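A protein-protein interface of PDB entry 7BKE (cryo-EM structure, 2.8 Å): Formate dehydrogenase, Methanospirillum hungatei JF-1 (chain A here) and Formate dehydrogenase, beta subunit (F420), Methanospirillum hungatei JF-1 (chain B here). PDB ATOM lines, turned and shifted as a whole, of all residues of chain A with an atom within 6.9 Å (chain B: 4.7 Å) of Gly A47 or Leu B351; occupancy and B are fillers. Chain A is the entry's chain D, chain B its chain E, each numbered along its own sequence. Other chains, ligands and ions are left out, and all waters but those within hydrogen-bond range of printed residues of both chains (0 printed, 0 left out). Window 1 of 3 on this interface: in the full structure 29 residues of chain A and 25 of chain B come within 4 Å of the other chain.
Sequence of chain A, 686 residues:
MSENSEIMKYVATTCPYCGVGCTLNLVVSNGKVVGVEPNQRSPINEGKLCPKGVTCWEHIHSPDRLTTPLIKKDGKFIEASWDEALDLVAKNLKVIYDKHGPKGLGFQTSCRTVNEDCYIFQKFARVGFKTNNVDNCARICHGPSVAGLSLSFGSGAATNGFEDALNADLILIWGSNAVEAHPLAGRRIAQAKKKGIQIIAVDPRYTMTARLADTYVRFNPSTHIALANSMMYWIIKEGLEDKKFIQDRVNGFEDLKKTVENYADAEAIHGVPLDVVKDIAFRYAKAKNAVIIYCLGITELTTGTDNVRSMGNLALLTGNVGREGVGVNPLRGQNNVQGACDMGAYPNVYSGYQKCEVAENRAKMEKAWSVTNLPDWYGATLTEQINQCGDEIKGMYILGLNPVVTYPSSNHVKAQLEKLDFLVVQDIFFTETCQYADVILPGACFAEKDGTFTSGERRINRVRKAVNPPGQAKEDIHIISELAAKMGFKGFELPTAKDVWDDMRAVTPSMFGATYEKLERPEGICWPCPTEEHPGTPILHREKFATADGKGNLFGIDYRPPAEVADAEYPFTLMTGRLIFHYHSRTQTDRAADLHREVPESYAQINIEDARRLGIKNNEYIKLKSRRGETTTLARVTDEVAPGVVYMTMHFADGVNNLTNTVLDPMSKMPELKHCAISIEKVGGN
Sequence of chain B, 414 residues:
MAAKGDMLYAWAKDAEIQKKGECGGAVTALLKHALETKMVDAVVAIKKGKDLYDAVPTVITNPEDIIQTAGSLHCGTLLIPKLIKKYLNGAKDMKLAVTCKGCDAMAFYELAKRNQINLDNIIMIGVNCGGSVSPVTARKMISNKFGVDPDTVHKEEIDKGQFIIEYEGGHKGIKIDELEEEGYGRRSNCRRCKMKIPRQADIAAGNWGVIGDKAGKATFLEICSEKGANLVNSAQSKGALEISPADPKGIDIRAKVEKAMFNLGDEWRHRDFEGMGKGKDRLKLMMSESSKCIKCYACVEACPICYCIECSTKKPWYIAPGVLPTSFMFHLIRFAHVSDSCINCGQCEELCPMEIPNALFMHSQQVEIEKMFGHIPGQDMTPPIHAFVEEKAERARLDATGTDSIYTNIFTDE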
ATOM      1  N   THR A  23       8.404  -1.352  12.379  1.00  0.00           N
ATOM      2  CA  THR A  23       7.213  -2.055  11.944  1.00  0.00           C
ATOM      3  C   THR A  23       6.609  -1.334  10.756  1.00  0.00           C
ATOM      4  O   THR A  23       6.625  -0.105  10.693  1.00  0.00           O
ATOM      5  CB  THR A  23       6.194  -2.150  13.071  1.00  0.00           C
ATOM      6  OG1 THR A  23       6.845  -2.632  14.248  1.00  0.00           O
ATOM      7  CG2 THR A  23       5.091  -3.100  12.709  1.00  0.00           C
ATOM      8  N   GLU A  37       3.197   0.479   3.723  1.00  0.00           N
ATOM      9  CA  GLU A  37       2.394   1.560   4.316  1.00  0.00           C
ATOM     10  C   GLU A  37       2.900   1.796   5.742  1.00  0.00           C
ATOM     11  O   GLU A  37       3.553   0.893   6.257  1.00  0.00           O
ATOM     12  CB  GLU A  37       0.913   1.312   4.131  1.00  0.00           C
ATOM     13  CG  GLU A  37       0.424   1.696   2.750  1.00  0.00           C
ATOM     14  CD  GLU A  37       0.843   3.060   2.221  1.00  0.00           C
ATOM     15  OE1 GLU A  37       1.211   3.145   1.034  1.00  0.00           O
ATOM     16  OE2 GLU A  37       0.781   4.042   2.986  1.00  0.00           O
ATOM     17  N   PRO A  38       2.756   2.986   6.364  1.00  0.00           N
ATOM     18  CA  PRO A  38       3.136   3.186   7.760  1.00  0.00           C
ATOM     19  C   PRO A  38       2.240   2.410   8.706  1.00  0.00           C
ATOM     20  O   PRO A  38       1.056   2.193   8.447  1.00  0.00           O
ATOM     21  CB  PRO A  38       2.957   4.693   7.950  1.00  0.00           C
ATOM     22  CG  PRO A  38       1.970   5.081   6.918  1.00  0.00           C
ATOM     23  CD  PRO A  38       2.288   4.235   5.746  1.00  0.00           C
ATOM     24  N   ASN A  39       2.825   1.997   9.825  1.00  0.00           N
ATOM     25  CA  ASN A  39       2.093   1.416  10.943  1.00  0.00           C
ATOM     26  C   ASN A  39       2.299   2.357  12.123  1.00  0.00           C
ATOM     27  O   ASN A  39       3.303   2.265  12.830  1.00  0.00           O
ATOM     28  CB  ASN A  39       2.572   0.022  11.253  1.00  0.00           C
ATOM     29  CG  ASN A  39       1.598  -0.755  12.098  1.00  0.00           C
ATOM     30  OD1 ASN A  39       0.593  -0.222  12.550  1.00  0.00           O
ATOM     31  ND2 ASN A  39       1.893  -2.017  12.321  1.00  0.00           N
ATOM     32  N   GLN A  40       1.349   3.268  12.329  1.00  0.00           N
ATOM     33  CA  GLN A  40       1.496   4.273  13.372  1.00  0.00           C
ATOM     34  C   GLN A  40       1.364   3.703  14.768  1.00  0.00           C
ATOM     35  O   GLN A  40       1.697   4.395  15.732  1.00  0.00           O
ATOM     36  CB  GLN A  40       0.467   5.381  13.184  1.00  0.00           C
ATOM     37  CG  GLN A  40       0.747   6.288  12.022  1.00  0.00           C
ATOM     38  CD  GLN A  40      -0.054   5.911  10.814  1.00  0.00           C
ATOM     39  OE1 GLN A  40      -0.526   4.787  10.700  1.00  0.00           O
ATOM     40  NE2 GLN A  40      -0.225   6.854   9.903  1.00  0.00           N
ATOM     41  N   ARG A  41       0.886   2.473  14.904  1.00  0.00           N
ATOM     42  CA  ARG A  41       0.711   1.890  16.224  1.00  0.00           C
ATOM     43  C   ARG A  41       2.044   1.511  16.855  1.00  0.00           C
ATOM     44  O   ARG A  41       2.162   1.494  18.082  1.00  0.00           O
ATOM     45  CB  ARG A  41      -0.204   0.678  16.115  1.00  0.00           C
ATOM     46  CG  ARG A  41      -0.393  -0.088  17.386  1.00  0.00           C
ATOM     47  CD  ARG A  41      -0.944   0.785  18.475  1.00  0.00           C
ATOM     48  NE  ARG A  41      -1.236   0.000  19.658  1.00  0.00           N
ATOM     49  CZ  ARG A  41      -0.357  -0.252  20.615  1.00  0.00           C
ATOM     50  NH1 ARG A  41       0.870   0.233  20.539  1.00  0.00           N
ATOM     51  NH2 ARG A  41      -0.713  -0.985  21.653  1.00  0.00           N
ATOM     52  N   SER A  42       3.087   1.247  16.092  1.00  0.00           N
ATOM     53  CA  SER A  42       4.350   0.710  16.647  1.00  0.00           C
ATOM     54  C   SER A  42       5.079   1.622  17.607  1.00  0.00           C
ATOM     55  O   SER A  42       5.278   2.775  17.292  1.00  0.00           O
ATOM     56  CB  SER A  42       5.267   0.334  15.571  1.00  0.00           C
ATOM     57  OG  SER A  42       6.414  -0.307  16.096  1.00  0.00           O
ATOM     58  N   ILE A  44       8.325   1.330  18.364  1.00  0.00           N
ATOM     59  CA  ILE A  44       9.736   1.508  17.907  1.00  0.00           C
ATOM     60  C   ILE A  44       9.876   2.689  16.973  1.00  0.00           C
ATOM     61  O   ILE A  44      10.750   3.515  17.199  1.00  0.00           O
ATOM     62  CB  ILE A  44      10.189   0.227  17.187  1.00  0.00           C
ATOM     63  CG1 ILE A  44      10.009  -1.012  18.065  1.00  0.00           C
ATOM     64  CG2 ILE A  44      11.611   0.355  16.676  1.00  0.00           C
ATOM     65  CD1 ILE A  44       9.310  -2.147  17.377  1.00  0.00           C
ATOM     66  N   ASN A  45       9.024   2.762  15.977  1.00  0.00           N
ATOM     67  CA  ASN A  45       9.019   3.831  14.972  1.00  0.00           C
ATOM     68  C   ASN A  45       7.557   4.168  14.980  1.00  0.00           C
ATOM     69  O   ASN A  45       6.763   3.268  15.055  1.00  0.00           O
ATOM     70  CB  ASN A  45       9.350   3.216  13.624  1.00  0.00           C
ATOM     71  CG  ASN A  45       8.415   2.140  13.121  1.00  0.00           C
ATOM     72  OD1 ASN A  45       8.098   1.202  13.836  1.00  0.00           O
ATOM     73  ND2 ASN A  45       7.981   2.258  11.882  1.00  0.00           N
ATOM     74  N   GLU A  46       7.172   5.405  15.024  1.00  0.00           N
ATOM     75  CA  GLU A  46       5.719   5.562  15.082  1.00  0.00           C
ATOM     76  C   GLU A  46       5.181   5.704  13.672  1.00  0.00           C
ATOM     77  O   GLU A  46       4.518   6.708  13.393  1.00  0.00           O
ATOM     78  CB  GLU A  46       5.411   6.627  16.112  1.00  0.00           C
ATOM     79  CG  GLU A  46       5.596   6.135  17.531  1.00  0.00           C
ATOM     80  CD  GLU A  46       6.939   6.457  18.154  1.00  0.00           C
ATOM     81  OE1 GLU A  46       7.699   7.177  17.519  1.00  0.00           O
ATOM     82  OE2 GLU A  46       7.219   5.981  19.269  1.00  0.00           O
ATOM     83  N   GLY A  47       5.365   4.694  12.842  1.00  0.00           N
ATOM     84  CA  GLY A  47       4.922   4.770  11.441  1.00  0.00           C
ATOM     85  C   GLY A  47       5.954   5.384  10.544  1.00  0.00           C
ATOM     86  O   GLY A  47       5.670   5.540   9.369  1.00  0.00           O
ATOM     87  N   LYS A  48       7.114   5.704  11.082  1.00  0.00           N
ATOM     88  CA  LYS A  48       8.162   6.404  10.335  1.00  0.00           C
ATOM     89  C   LYS A  48       9.140   5.357   9.861  1.00  0.00           C
ATOM     90  O   LYS A  48       9.320   4.403  10.568  1.00  0.00           O
ATOM     91  CB  LYS A  48       8.779   7.470  11.232  1.00  0.00           C
ATOM     92  CG  LYS A  48       7.781   8.378  11.925  1.00  0.00           C
ATOM     93  CD  LYS A  48       8.372   9.103  13.091  1.00  0.00           C
ATOM     94  CE  LYS A  48       7.408  10.103  13.681  1.00  0.00           C
ATOM     95  NZ  LYS A  48       7.680  11.468  13.189  1.00  0.00           N
ATOM     96  N   LEU A  49       9.627   5.471   8.641  1.00  0.00           N
ATOM     97  CA  LEU A  49      10.536   4.472   8.058  1.00  0.00           C
ATOM     98  C   LEU A  49      11.579   5.241   7.279  1.00  0.00           C
ATOM     99  O   LEU A  49      11.282   6.355   6.912  1.00  0.00           O
ATOM    100  CB  LEU A  49       9.749   3.546   7.129  1.00  0.00           C
ATOM    101  CG  LEU A  49       8.711   2.627   7.759  1.00  0.00           C
ATOM    102  CD1 LEU A  49       7.678   2.224   6.729  1.00  0.00           C
ATOM    103  CD2 LEU A  49       9.373   1.401   8.349  1.00  0.00           C
ATOM    104  N   LEU A 184      16.290   5.409  12.349  1.00  0.00           N
ATOM    105  CA  LEU A 184      15.263   5.584  13.361  1.00  0.00           C
ATOM    106  C   LEU A 184      15.752   5.239  14.753  1.00  0.00           C
ATOM    107  O   LEU A 184      14.967   5.286  15.702  1.00  0.00           O
ATOM    108  CB  LEU A 184      14.009   4.793  13.016  1.00  0.00           C
ATOM    109  CG  LEU A 184      13.190   5.562  11.981  1.00  0.00           C
ATOM    110  CD1 LEU A 184      13.782   5.535  10.604  1.00  0.00           C
ATOM    111  CD2 LEU A 184      11.817   5.063  11.940  1.00  0.00           C
ATOM    112  N   ALA B 298       9.082  10.292   2.440  1.00  0.00           N
ATOM    113  CA  ALA B 298       7.788   9.946   3.011  1.00  0.00           C
ATOM    114  C   ALA B 298       6.816  11.109   2.913  1.00  0.00           C
ATOM    115  O   ALA B 298       5.624  10.907   2.673  1.00  0.00           O
ATOM    116  CB  ALA B 298       7.952   9.508   4.460  1.00  0.00           C
ATOM    117  N   ALA B 302       3.323  10.695   0.943  1.00  0.00           N
ATOM    118  CA  ALA B 302       2.120  10.794   1.745  1.00  0.00           C
ATOM    119  C   ALA B 302       1.290  12.025   1.445  1.00  0.00           C
ATOM    120  O   ALA B 302       0.099  12.027   1.750  1.00  0.00           O
ATOM    121  CB  ALA B 302       2.485  10.796   3.225  1.00  0.00           C
ATOM    122  N   GLN B 347       0.212  14.628   7.418  1.00  0.00           N
ATOM    123  CA  GLN B 347       0.882  13.370   7.119  1.00  0.00           C
ATOM    124  C   GLN B 347       2.373  13.569   6.942  1.00  0.00           C
ATOM    125  O   GLN B 347       3.177  12.746   7.394  1.00  0.00           O
ATOM    126  CB  GLN B 347       0.277  12.741   5.869  1.00  0.00           C
ATOM    127  CG  GLN B 347      -1.192  12.440   5.959  1.00  0.00           C
ATOM    128  CD  GLN B 347      -1.528  11.539   7.113  1.00  0.00           C
ATOM    129  OE1 GLN B 347      -0.824  10.578   7.385  1.00  0.00           O
ATOM    130  NE2 GLN B 347      -2.613  11.841   7.803  1.00  0.00           N
ATOM    131  N   CYS B 348       2.762  14.662   6.298  1.00  0.00           N
ATOM    132  CA  CYS B 348       4.173  14.973   6.123  1.00  0.00           C
ATOM    133  C   CYS B 348       4.866  15.157   7.460  1.00  0.00           C
ATOM    134  O   CYS B 348       6.020  14.755   7.627  1.00  0.00           O
ATOM    135  CB  CYS B 348       4.325  16.230   5.282  1.00  0.00           C
ATOM    136  SG  CYS B 348       3.448  17.628   5.934  1.00  0.00           S
ATOM    137  N   GLU B 349       4.194  15.796   8.411  1.00  0.00           N
ATOM    138  CA  GLU B 349       4.807  16.021   9.712  1.00  0.00           C
ATOM    139  C   GLU B 349       4.923  14.730  10.492  1.00  0.00           C
ATOM    140  O   GLU B 349       5.944  14.476  11.136  1.00  0.00           O
ATOM    141  CB  GLU B 349       4.010  17.042  10.512  1.00  0.00           C
ATOM    142  CG  GLU B 349       4.712  17.491  11.772  1.00  0.00           C
ATOM    143  CD  GLU B 349       4.203  18.818  12.298  1.00  0.00           C
ATOM    144  OE1 GLU B 349       3.057  19.199  11.992  1.00  0.00           O
ATOM    145  OE2 GLU B 349       4.949  19.486  13.033  1.00  0.00           O
ATOM    146  N   GLU B 350       3.899  13.896  10.444  1.00  0.00           N
ATOM    147  CA  GLU B 350       3.872  12.739  11.313  1.00  0.00           C
ATOM    148  C   GLU B 350       4.583  11.522  10.747  1.00  0.00           C
ATOM    149  O   GLU B 350       4.832  10.580  11.499  1.00  0.00           O
ATOM    150  CB  GLU B 350       2.440  12.370  11.644  1.00  0.00           C
ATOM    151  CG  GLU B 350       1.801  11.492  10.645  1.00  0.00           C
ATOM    152  CD  GLU B 350       0.375  11.242  10.996  1.00  0.00           C
ATOM    153  OE1 GLU B 350       0.013  11.543  12.150  1.00  0.00           O
ATOM    154  OE2 GLU B 350      -0.384  10.750  10.138  1.00  0.00           O
ATOM    155  N   LEU B 351       4.925  11.509   9.463  1.00  0.00           N
ATOM    156  CA  LEU B 351       5.678  10.395   8.905  1.00  0.00           C
ATOM    157  C   LEU B 351       7.156  10.699   8.736  1.00  0.00           C
ATOM    158  O   LEU B 351       7.859   9.918   8.100  1.00  0.00           O
ATOM    159  CB  LEU B 351       5.087   9.976   7.567  1.00  0.00           C
ATOM    160  CG  LEU B 351       3.669   9.431   7.600  1.00  0.00           C
ATOM    161  CD1 LEU B 351       3.345   8.800   6.287  1.00  0.00           C
ATOM    162  CD2 LEU B 351       3.525   8.434   8.710  1.00  0.00           C
ATOM    163  N   CYS B 352       7.647  11.796   9.289  1.00  0.00           N
ATOM    164  CA  CYS B 352       9.029  12.187   9.083  1.00  0.00           C
ATOM    165  C   CYS B 352       9.925  11.513  10.112  1.00  0.00           C
ATOM    166  O   CYS B 352       9.755  11.751  11.310  1.00  0.00           O
ATOM    167  CB  CYS B 352       9.176  13.691   9.173  1.00  0.00           C
ATOM    168  SG  CYS B 352      10.806  14.310   8.809  1.00  0.00           S
ATOM    169  N   PRO B 353      10.888  10.688   9.699  1.00  0.00           N
ATOM    170  CA  PRO B 353      11.784  10.057  10.669  1.00  0.00           C
ATOM    171  C   PRO B 353      12.628  11.033  11.435  1.00  0.00           C
ATOM    172  O   PRO B 353      13.171  10.663  12.475  1.00  0.00           O
ATOM    173  CB  PRO B 353      12.665   9.155   9.805  1.00  0.00           C
ATOM    174  CG  PRO B 353      12.011   9.057   8.546  1.00  0.00           C
ATOM    175  CD  PRO B 353      11.161  10.230   8.338  1.00  0.00           C
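O of Glu B350 sits close to NZ of Lys A48 (3.4 Å). The side-chain amino group (NZ) of Lys A48 lies within hydrogen-bond range of the backbone carbonyl oxygen (O) of Cys B352, at 2.8 Å.
The side-chain carboxylate (OE2) of Glu B350 lies close to the side-chain amide oxygen (OE1) of Gln B347 (2.8 Å). The backbone carbonyl oxygen (O) of Asn A39 lies within hydrogen-bond range of the backbone NH (N) of Gly A47. O of Lys A48 lies within hydrogen-bond range of ND2 of Asn A45 (2.8 Å).
Among the printed residues, pairs that only touch across the chains: Leu A49 with Pro B353, Gly A47 with Leu B351, Pro A38 with Leu B351, Leu A184 with Pro B353, Gln A40 with Glu B350 and Lys A48 with Leu B351.
Of the printed residues of chain B, Pro A38 touches Leu B351 (3.9 Å). Printed residues of chain B within 4 Å of Gln A40: Glu B350. Arg A41 touches none of the printed residues of chain B. Ile A44 touches none of the printed residues of chain B. Of the printed residues of chain B, Gly A47 touches Leu B351 (3.7 Å). Printed residues of chain B within 4 Å of Lys A48: Glu B350, Leu B351 and Cys B352. Of the printed residues of chain A, Glu B350 touches Gln A40 and Lys A48. Of the printed residues of chain A, Leu B351 touches Pro A38, Gly A47 and Lys A48. Of the printed residues of chain A, Pro B353 touches Leu A49 (3.2 Å) and Leu A184 (3.9 Å). The nearest printed residue of chain B that does not touch Lys A48 is Pro B353 (4.005 Å).
Printed residues of chain B that touch a printed residue of chain A: Glu B350, Leu B351, Cys B352 and Pro B353. Hydrophobic or aromatic side chains of chain A that line the printed part of chain B: Pro A38 and Leu A184.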
